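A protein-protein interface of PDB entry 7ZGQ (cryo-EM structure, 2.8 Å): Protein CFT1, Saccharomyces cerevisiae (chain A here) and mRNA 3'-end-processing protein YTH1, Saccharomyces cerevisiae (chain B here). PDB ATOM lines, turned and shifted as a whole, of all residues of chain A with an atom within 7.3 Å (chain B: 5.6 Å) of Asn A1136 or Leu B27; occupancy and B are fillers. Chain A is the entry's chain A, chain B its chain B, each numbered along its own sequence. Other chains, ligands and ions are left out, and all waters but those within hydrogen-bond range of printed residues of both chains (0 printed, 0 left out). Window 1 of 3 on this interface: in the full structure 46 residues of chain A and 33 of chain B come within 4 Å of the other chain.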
ATOM      1  N   GLU A1092      -7.555  20.468  31.709  1.00  0.00           N
ATOM      2  CA  GLU A1092      -8.391  21.538  32.234  1.00  0.00           C
ATOM      3  C   GLU A1092      -8.845  22.435  31.091  1.00  0.00           C
ATOM      4  O   GLU A1092      -8.041  22.815  30.234  1.00  0.00           O
ATOM      5  CB  GLU A1092      -7.640  22.350  33.292  1.00  0.00           C
ATOM      6  CG  GLU A1092      -6.329  22.951  32.821  1.00  0.00           C
ATOM      7  CD  GLU A1092      -6.458  24.417  32.468  1.00  0.00           C
ATOM      8  OE1 GLU A1092      -7.543  24.990  32.700  1.00  0.00           O
ATOM      9  OE2 GLU A1092      -5.474  24.998  31.962  1.00  0.00           O
ATOM     10  N   VAL A1093     -10.136  22.754  31.071  1.00  0.00           N
ATOM     11  CA  VAL A1093     -10.734  23.572  30.020  1.00  0.00           C
ATOM     12  C   VAL A1093     -11.420  24.749  30.699  1.00  0.00           C
ATOM     13  O   VAL A1093     -12.511  24.601  31.265  1.00  0.00           O
ATOM     14  CB  VAL A1093     -11.720  22.782  29.153  1.00  0.00           C
ATOM     15  CG1 VAL A1093     -11.474  23.065  27.681  1.00  0.00           C
ATOM     16  CG2 VAL A1093     -11.619  21.294  29.445  1.00  0.00           C
ATOM     17  N   SER A1094     -10.786  25.920  30.641  1.00  0.00           N
ATOM     18  CA  SER A1094     -11.372  27.172  31.117  1.00  0.00           C
ATOM     19  C   SER A1094     -11.820  27.064  32.573  1.00  0.00           C
ATOM     20  O   SER A1094     -12.935  27.440  32.938  1.00  0.00           O
ATOM     21  CB  SER A1094     -12.531  27.601  30.218  1.00  0.00           C
ATOM     22  OG  SER A1094     -12.083  27.859  28.899  1.00  0.00           O
ATOM     23  N   SER A1133      -5.511  21.357  25.873  1.00  0.00           N
ATOM     24  CA  SER A1133      -6.501  22.422  25.802  1.00  0.00           C
ATOM     25  C   SER A1133      -5.818  23.754  25.537  1.00  0.00           C
ATOM     26  O   SER A1133      -4.764  24.048  26.107  1.00  0.00           O
ATOM     27  CB  SER A1133      -7.322  22.512  27.091  1.00  0.00           C
ATOM     28  OG  SER A1133      -6.484  22.633  28.225  1.00  0.00           O
ATOM     29  N   PHE A1134      -6.427  24.554  24.665  1.00  0.00           N
ATOM     30  CA  PHE A1134      -5.991  25.918  24.378  1.00  0.00           C
ATOM     31  C   PHE A1134      -7.201  26.819  24.605  1.00  0.00           C
ATOM     32  O   PHE A1134      -7.950  27.122  23.674  1.00  0.00           O
ATOM     33  CB  PHE A1134      -5.448  26.043  22.960  1.00  0.00           C
ATOM     34  CG  PHE A1134      -4.650  27.292  22.728  1.00  0.00           C
ATOM     35  CD1 PHE A1134      -5.282  28.492  22.456  1.00  0.00           C
ATOM     36  CD2 PHE A1134      -3.269  27.267  22.787  1.00  0.00           C
ATOM     37  CE1 PHE A1134      -4.550  29.643  22.246  1.00  0.00           C
ATOM     38  CE2 PHE A1134      -2.532  28.414  22.576  1.00  0.00           C
ATOM     39  CZ  PHE A1134      -3.173  29.604  22.305  1.00  0.00           C
ATOM     40  N   GLY A1135      -7.384  27.253  25.849  1.00  0.00           N
ATOM     41  CA  GLY A1135      -8.587  27.970  26.215  1.00  0.00           C
ATOM     42  C   GLY A1135      -9.739  27.014  26.431  1.00  0.00           C
ATOM     43  O   GLY A1135      -9.656  26.119  27.276  1.00  0.00           O
ATOM     44  N   ASN A1136     -10.819  27.185  25.672  1.00  0.00           N
ATOM     45  CA  ASN A1136     -11.951  26.271  25.721  1.00  0.00           C
ATOM     46  C   ASN A1136     -11.949  25.279  24.564  1.00  0.00           C
ATOM     47  O   ASN A1136     -12.937  24.565  24.371  1.00  0.00           O
ATOM     48  CB  ASN A1136     -13.264  27.055  25.749  1.00  0.00           C
ATOM     49  CG  ASN A1136     -13.408  27.992  24.574  1.00  0.00           C
ATOM     50  OD1 ASN A1136     -12.460  28.215  23.821  1.00  0.00           O
ATOM     51  ND2 ASN A1136     -14.600  28.552  24.409  1.00  0.00           N
ATOM     52  N   LEU A1137     -10.867  25.220  23.796  1.00  0.00           N
ATOM     53  CA  LEU A1137     -10.718  24.240  22.731  1.00  0.00           C
ATOM     54  C   LEU A1137      -9.935  23.037  23.236  1.00  0.00           C
ATOM     55  O   LEU A1137      -9.051  23.161  24.087  1.00  0.00           O
ATOM     56  CB  LEU A1137     -10.010  24.855  21.523  1.00  0.00           C
ATOM     57  CG  LEU A1137     -10.670  26.085  20.901  1.00  0.00           C
ATOM     58  CD1 LEU A1137      -9.721  26.772  19.934  1.00  0.00           C
ATOM     59  CD2 LEU A1137     -11.963  25.704  20.204  1.00  0.00           C
ATOM     60  N   LEU A1138     -10.271  21.863  22.707  1.00  0.00           N
ATOM     61  CA  LEU A1138      -9.649  20.618  23.130  1.00  0.00           C
ATOM     62  C   LEU A1138      -9.284  19.785  21.913  1.00  0.00           C
ATOM     63  O   LEU A1138      -9.916  19.887  20.859  1.00  0.00           O
ATOM     64  CB  LEU A1138     -10.577  19.806  24.039  1.00  0.00           C
ATOM     65  CG  LEU A1138     -10.671  20.197  25.511  1.00  0.00           C
ATOM     66  CD1 LEU A1138     -11.995  19.725  26.084  1.00  0.00           C
ATOM     67  CD2 LEU A1138      -9.508  19.613  26.294  1.00  0.00           C
ATOM     68  N   PHE A1149     -11.120  17.535  17.199  1.00  0.00           N
ATOM     69  CA  PHE A1149     -11.113  18.893  17.726  1.00  0.00           C
ATOM     70  C   PHE A1149     -12.453  19.178  18.392  1.00  0.00           C
ATOM     71  O   PHE A1149     -13.509  18.966  17.786  1.00  0.00           O
ATOM     72  CB  PHE A1149     -10.845  19.897  16.603  1.00  0.00           C
ATOM     73  CG  PHE A1149     -10.487  21.269  17.083  1.00  0.00           C
ATOM     74  CD1 PHE A1149      -9.755  21.443  18.240  1.00  0.00           C
ATOM     75  CD2 PHE A1149     -10.872  22.386  16.365  1.00  0.00           C
ATOM     76  CE1 PHE A1149      -9.422  22.704  18.680  1.00  0.00           C
ATOM     77  CE2 PHE A1149     -10.541  23.650  16.799  1.00  0.00           C
ATOM     78  CZ  PHE A1149      -9.815  23.809  17.958  1.00  0.00           C
ATOM     79  N   ILE A1150     -12.411  19.653  19.637  1.00  0.00           N
ATOM     80  CA  ILE A1150     -13.603  19.826  20.460  1.00  0.00           C
ATOM     81  C   ILE A1150     -13.600  21.222  21.064  1.00  0.00           C
ATOM     82  O   ILE A1150     -12.571  21.692  21.562  1.00  0.00           O
ATOM     83  CB  ILE A1150     -13.687  18.759  21.577  1.00  0.00           C
ATOM     84  CG1 ILE A1150     -14.074  17.395  21.005  1.00  0.00           C
ATOM     85  CG2 ILE A1150     -14.679  19.168  22.652  1.00  0.00           C
ATOM     86  CD1 ILE A1150     -12.908  16.574  20.515  1.00  0.00           C
ATOM     87  N   GLY A1151     -14.749  21.884  21.021  1.00  0.00           N
ATOM     88  CA  GLY A1151     -14.940  23.164  21.688  1.00  0.00           C
ATOM     89  C   GLY A1151     -15.928  23.027  22.830  1.00  0.00           C
ATOM     90  O   GLY A1151     -16.895  22.269  22.731  1.00  0.00           O
ATOM     91  N   PHE A1152     -15.682  23.764  23.910  1.00  0.00           N
ATOM     92  CA  PHE A1152     -16.477  23.670  25.131  1.00  0.00           C
ATOM     93  C   PHE A1152     -17.074  25.031  25.463  1.00  0.00           C
ATOM     94  O   PHE A1152     -16.344  26.020  25.578  1.00  0.00           O
ATOM     95  CB  PHE A1152     -15.621  23.163  26.294  1.00  0.00           C
ATOM     96  CG  PHE A1152     -16.249  23.358  27.643  1.00  0.00           C
ATOM     97  CD1 PHE A1152     -17.350  22.612  28.024  1.00  0.00           C
ATOM     98  CD2 PHE A1152     -15.735  24.285  28.533  1.00  0.00           C
ATOM     99  CE1 PHE A1152     -17.929  22.789  29.268  1.00  0.00           C
ATOM    100  CE2 PHE A1152     -16.308  24.466  29.777  1.00  0.00           C
ATOM    101  CZ  PHE A1152     -17.406  23.717  30.144  1.00  0.00           C
ATOM    102  N   ASP A1153     -18.395  25.075  25.622  1.00  0.00           N
ATOM    103  CA  ASP A1153     -19.118  26.269  26.038  1.00  0.00           C
ATOM    104  C   ASP A1153     -19.596  26.104  27.475  1.00  0.00           C
ATOM    105  O   ASP A1153     -19.773  24.985  27.966  1.00  0.00           O
ATOM    106  CB  ASP A1153     -20.305  26.545  25.110  1.00  0.00           C
ATOM    107  CG  ASP A1153     -20.758  27.991  25.158  1.00  0.00           C
ATOM    108  OD1 ASP A1153     -19.951  28.881  24.817  1.00  0.00           O
ATOM    109  OD2 ASP A1153     -21.923  28.239  25.536  1.00  0.00           O
ATOM    110  N   ALA A1154     -19.813  27.234  28.152  1.00  0.00           N
ATOM    111  CA  ALA A1154     -19.979  27.232  29.604  1.00  0.00           C
ATOM    112  C   ALA A1154     -21.435  27.285  30.056  1.00  0.00           C
ATOM    113  O   ALA A1154     -21.890  26.378  30.758  1.00  0.00           O
ATOM    114  CB  ALA A1154     -19.199  28.399  30.220  1.00  0.00           C
ATOM    115  N   ARG A1158     -21.560  22.205  26.788  1.00  0.00           N
ATOM    116  CA  ARG A1158     -21.595  21.374  25.596  1.00  0.00           C
ATOM    117  C   ARG A1158     -20.175  21.031  25.165  1.00  0.00           C
ATOM    118  O   ARG A1158     -19.196  21.622  25.627  1.00  0.00           O
ATOM    119  CB  ARG A1158     -22.349  22.065  24.454  1.00  0.00           C
ATOM    120  CG  ARG A1158     -22.277  23.577  24.496  1.00  0.00           C
ATOM    121  CD  ARG A1158     -23.540  24.204  23.938  1.00  0.00           C
ATOM    122  NE  ARG A1158     -23.583  24.148  22.482  1.00  0.00           N
ATOM    123  CZ  ARG A1158     -23.303  25.169  21.684  1.00  0.00           C
ATOM    124  NH1 ARG A1158     -22.947  26.347  22.169  1.00  0.00           N
ATOM    125  NH2 ARG A1158     -23.384  25.003  20.367  1.00  0.00           N
ATOM    126  N   MET A1159     -20.079  20.059  24.261  1.00  0.00           N
ATOM    127  CA  MET A1159     -18.828  19.538  23.710  1.00  0.00           C
ATOM    128  C   MET A1159     -18.906  19.442  22.197  1.00  0.00           C
ATOM    129  O   MET A1159     -18.696  18.380  21.607  1.00  0.00           O
ATOM    130  CB  MET A1159     -18.455  18.184  24.303  1.00  0.00           C
ATOM    131  CG  MET A1159     -18.439  18.151  25.806  1.00  0.00           C
ATOM    132  SD  MET A1159     -16.902  17.377  26.329  1.00  0.00           S
ATOM    133  CE  MET A1159     -15.848  18.818  26.423  1.00  0.00           C
ATOM    134  N   LEU A1162     -15.762  19.843  16.591  1.00  0.00           N
ATOM    135  CA  LEU A1162     -15.423  20.778  15.527  1.00  0.00           C
ATOM    136  C   LEU A1162     -14.779  20.110  14.321  1.00  0.00           C
ATOM    137  O   LEU A1162     -14.945  20.595  13.198  1.00  0.00           O
ATOM    138  CB  LEU A1162     -14.499  21.871  16.068  1.00  0.00           C
ATOM    139  CG  LEU A1162     -14.979  22.536  17.359  1.00  0.00           C
ATOM    140  CD1 LEU A1162     -13.960  23.538  17.867  1.00  0.00           C
ATOM    141  CD2 LEU A1162     -16.328  23.200  17.150  1.00  0.00           C
ATOM    142  N   ALA B   9      -6.580  31.655  27.159  1.00  0.00           N
ATOM    143  CA  ALA B   9      -8.030  31.816  27.124  1.00  0.00           C
ATOM    144  C   ALA B   9      -8.467  32.771  26.020  1.00  0.00           C
ATOM    145  O   ALA B   9      -9.446  32.506  25.313  1.00  0.00           O
ATOM    146  CB  ALA B   9      -8.534  32.302  28.483  1.00  0.00           C
ATOM    147  N   TYR B  11      -7.247  34.305  22.693  1.00  0.00           N
ATOM    148  CA  TYR B  11      -6.304  34.322  21.590  1.00  0.00           C
ATOM    149  C   TYR B  11      -7.027  34.687  20.300  1.00  0.00           C
ATOM    150  O   TYR B  11      -8.147  34.219  20.059  1.00  0.00           O
ATOM    151  CB  TYR B  11      -5.610  32.962  21.432  1.00  0.00           C
ATOM    152  CG  TYR B  11      -4.443  32.989  20.474  1.00  0.00           C
ATOM    153  CD1 TYR B  11      -4.636  32.829  19.109  1.00  0.00           C
ATOM    154  CD2 TYR B  11      -3.148  33.188  20.936  1.00  0.00           C
ATOM    155  CE1 TYR B  11      -3.576  32.864  18.233  1.00  0.00           C
ATOM    156  CE2 TYR B  11      -2.080  33.221  20.064  1.00  0.00           C
ATOM    157  CZ  TYR B  11      -2.300  33.060  18.714  1.00  0.00           C
ATOM    158  OH  TYR B  11      -1.240  33.090  17.840  1.00  0.00           O
ATOM    159  N   PHE B  13      -7.957  33.929  17.148  1.00  0.00           N
ATOM    160  CA  PHE B  13      -8.083  32.903  16.123  1.00  0.00           C
ATOM    161  C   PHE B  13      -8.900  33.425  14.948  1.00  0.00           C
ATOM    162  O   PHE B  13      -9.927  34.088  15.130  1.00  0.00           O
ATOM    163  CB  PHE B  13      -8.735  31.646  16.699  1.00  0.00           C
ATOM    164  CG  PHE B  13      -7.803  30.803  17.519  1.00  0.00           C
ATOM    165  CD1 PHE B  13      -6.560  30.443  17.027  1.00  0.00           C
ATOM    166  CD2 PHE B  13      -8.169  30.368  18.780  1.00  0.00           C
ATOM    167  CE1 PHE B  13      -5.701  29.667  17.780  1.00  0.00           C
ATOM    168  CE2 PHE B  13      -7.315  29.592  19.536  1.00  0.00           C
ATOM    169  CZ  PHE B  13      -6.080  29.242  19.035  1.00  0.00           C
ATOM    170  N   PHE B  15     -10.721  31.828  12.909  1.00  0.00           N
ATOM    171  CA  PHE B  15     -11.963  31.101  12.682  1.00  0.00           C
ATOM    172  C   PHE B  15     -13.032  31.438  13.712  1.00  0.00           C
ATOM    173  O   PHE B  15     -14.049  30.742  13.784  1.00  0.00           O
ATOM    174  CB  PHE B  15     -11.702  29.593  12.662  1.00  0.00           C
ATOM    175  CG  PHE B  15     -10.917  29.094  13.839  1.00  0.00           C
ATOM    176  CD1 PHE B  15     -11.540  28.834  15.048  1.00  0.00           C
ATOM    177  CD2 PHE B  15      -9.555  28.878  13.735  1.00  0.00           C
ATOM    178  CE1 PHE B  15     -10.819  28.372  16.130  1.00  0.00           C
ATOM    179  CE2 PHE B  15      -8.830  28.417  14.815  1.00  0.00           C
ATOM    180  CZ  PHE B  15      -9.463  28.162  16.013  1.00  0.00           C
ATOM    181  N   GLU B  16     -12.816  32.477  14.517  1.00  0.00           N
ATOM    182  CA  GLU B  16     -13.835  32.902  15.473  1.00  0.00           C
ATOM    183  C   GLU B  16     -15.171  33.252  14.825  1.00  0.00           C
ATOM    184  O   GLU B  16     -16.207  32.802  15.345  1.00  0.00           O
ATOM    185  CB  GLU B  16     -13.306  34.083  16.296  1.00  0.00           C
ATOM    186  N   LEU B  19     -16.783  30.009  13.978  1.00  0.00           N
ATOM    187  CA  LEU B  19     -17.168  29.289  15.185  1.00  0.00           C
ATOM    188  C   LEU B  19     -18.363  29.930  15.874  1.00  0.00           C
ATOM    189  O   LEU B  19     -19.041  29.263  16.660  1.00  0.00           O
ATOM    190  CB  LEU B  19     -15.983  29.213  16.149  1.00  0.00           C
ATOM    191  CG  LEU B  19     -15.739  27.867  16.831  1.00  0.00           C
ATOM    192  CD1 LEU B  19     -15.853  26.729  15.832  1.00  0.00           C
ATOM    193  CD2 LEU B  19     -14.379  27.856  17.505  1.00  0.00           C
ATOM    194  N   PHE B  25     -20.886  29.228  18.971  1.00  0.00           N
ATOM    195  CA  PHE B  25     -19.764  29.020  19.875  1.00  0.00           C
ATOM    196  C   PHE B  25     -18.845  30.234  19.877  1.00  0.00           C
ATOM    197  O   PHE B  25     -18.579  30.827  18.829  1.00  0.00           O
ATOM    198  CB  PHE B  25     -18.978  27.770  19.475  1.00  0.00           C
ATOM    199  CG  PHE B  25     -17.990  27.324  20.502  1.00  0.00           C
ATOM    200  CD1 PHE B  25     -18.323  27.323  21.844  1.00  0.00           C
ATOM    201  CD2 PHE B  25     -16.726  26.905  20.129  1.00  0.00           C
ATOM    202  CE1 PHE B  25     -17.415  26.915  22.793  1.00  0.00           C
ATOM    203  CE2 PHE B  25     -15.812  26.495  21.074  1.00  0.00           C
ATOM    204  CZ  PHE B  25     -16.156  26.499  22.409  1.00  0.00           C
ATOM    205  N   SER B  26     -18.357  30.599  21.059  1.00  0.00           N
ATOM    206  CA  SER B  26     -17.435  31.714  21.206  1.00  0.00           C
ATOM    207  C   SER B  26     -16.208  31.265  21.986  1.00  0.00           C
ATOM    208  O   SER B  26     -16.281  30.357  22.820  1.00  0.00           O
ATOM    209  CB  SER B  26     -18.092  32.905  21.911  1.00  0.00           C
ATOM    210  OG  SER B  26     -17.168  33.961  22.096  1.00  0.00           O
ATOM    211  N   LEU B  27     -15.077  31.913  21.705  1.00  0.00           N
ATOM    212  CA  LEU B  27     -13.834  31.598  22.398  1.00  0.00           C
ATOM    213  C   LEU B  27     -13.884  31.945  23.879  1.00  0.00           C
ATOM    214  O   LEU B  27     -13.033  31.469  24.638  1.00  0.00           O
ATOM    215  CB  LEU B  27     -12.648  32.318  21.742  1.00  0.00           C
ATOM    216  CG  LEU B  27     -12.131  31.910  20.354  1.00  0.00           C
ATOM    217  CD1 LEU B  27     -11.480  30.534  20.411  1.00  0.00           C
ATOM    218  CD2 LEU B  27     -13.187  31.963  19.255  1.00  0.00           C
ATOM    219  N   ASP B  28     -14.852  32.755  24.307  1.00  0.00           N
ATOM    220  CA  ASP B  28     -15.030  33.054  25.719  1.00  0.00           C
ATOM    221  C   ASP B  28     -16.171  32.208  26.254  1.00  0.00           C
ATOM    222  O   ASP B  28     -17.333  32.463  25.906  1.00  0.00           O
ATOM    223  CB  ASP B  28     -15.325  34.538  25.925  1.00  0.00           C
ATOM    224  CG  ASP B  28     -14.274  35.435  25.301  1.00  0.00           C
ATOM    225  OD1 ASP B  28     -13.076  35.095  25.381  1.00  0.00           O
ATOM    226  OD2 ASP B  28     -14.649  36.482  24.731  1.00  0.00           O
ATOM    227  N   PRO B  29     -15.905  31.200  27.083  1.00  0.00           N
ATOM    228  CA  PRO B  29     -16.997  30.354  27.585  1.00  0.00           C
ATOM    229  C   PRO B  29     -17.917  31.093  28.545  1.00  0.00           C
ATOM    230  O   PRO B  29     -19.142  31.027  28.414  1.00  0.00           O
ATOM    231  CB  PRO B  29     -16.258  29.204  28.282  1.00  0.00           C
ATOM    232  CG  PRO B  29     -14.926  29.764  28.631  1.00  0.00           C
ATOM    233  CD  PRO B  29     -14.586  30.746  27.552  1.00  0.00           C
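The backbone carbonyl oxygen of Ser B26 is in hydrogen-bond range of the side-chain amide nitrogen of Asn A1136.
The side-chain amide nitrogen (ND2) of Asn A1136 lies within hydrogen-bond range of the backbone carbonyl oxygen (O) of Leu B27 (3.3 Å).
The side-chain hydroxyl of Ser A1094 sits at hydrogen-bond distance from the backbone carbonyl oxygen of Gly A1135, 3.4 Å away.
The backbone carbonyl oxygen of Asn A1136 lies within hydrogen-bond range of the backbone NH of Phe A1152 (2.9 Å).
O of Phe A1149 is in hydrogen-bond range of N of Leu A1162, 2.7 Å away.
OD2 of Asp A1153 lies within salt-bridge range of NH1 of Arg A1158, 3.996 Å away.
The backbone carbonyl oxygen (O) of Leu B19 sits at hydrogen-bond distance from the backbone NH (N) of Phe B25 (3.0 Å).
The backbone NH (N) of Asp B28 lies close to the side-chain hydroxyl (OG) of Ser B26, at 3.4 Å.
Ser A1094 touches Pro B29.
Phe A1134 touches Tyr B11 (CE1 to CB, 3.6 Å).
Phe A1134 touches Phe B13.
ND2 of Asn A1136 touches CZ of Phe B25 (3.3 Å).
Pro B29 touches Asn A1136 (CD to ND2, 3.8 Å).
CA of Gly A1151 touches CE2 of Phe B25, 3.5 Å away.
CE1 of Phe B25 touches O of Phe A1152, 3.1 Å away.
Asp A1153 touches Phe B25 (N to CE1, 3.5 Å).
O of Pro B29 touches CB of Ala A1154 (3.2 Å).
CD2 of Leu A1162 touches CD1 of Leu B19, at 3.8 Å.
Asn A1136 touches four residues of chain B.
Arg A1158 touches none of the printed residues of chain B.
Printed residues of chain A within 4 Å of Leu B19: Leu A1162.
Of the printed residues of chain A, Phe B25 touches Asn A1136, Gly A1151, Phe A1152 and Asp A1153.
Leu B27 touches just one residue of chain A: Asn A1136.
The nearest residue of chain A that does not touch Leu B27 is Leu A1137 (4.2 Å).
Printed residues of chain B that touch a printed residue of chain A: Ala B9, Tyr B11, Phe B13, Leu B19, Phe B25, Ser B26, Leu B27 and Pro B29.
Hydrophobic or aromatic side chains of chain B within 4 Å of the printed part of chain A: Tyr B11, Phe B13, Leu B19, Phe B25 and Pro B29.
Along chain B the printed residues that touch a printed residue of chain A span positions 9 to 29.
Among the printed residues, no Asp or Glu carboxylate lies within 4 Å of a Lys or Arg side-chain nitrogen of the other chain.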
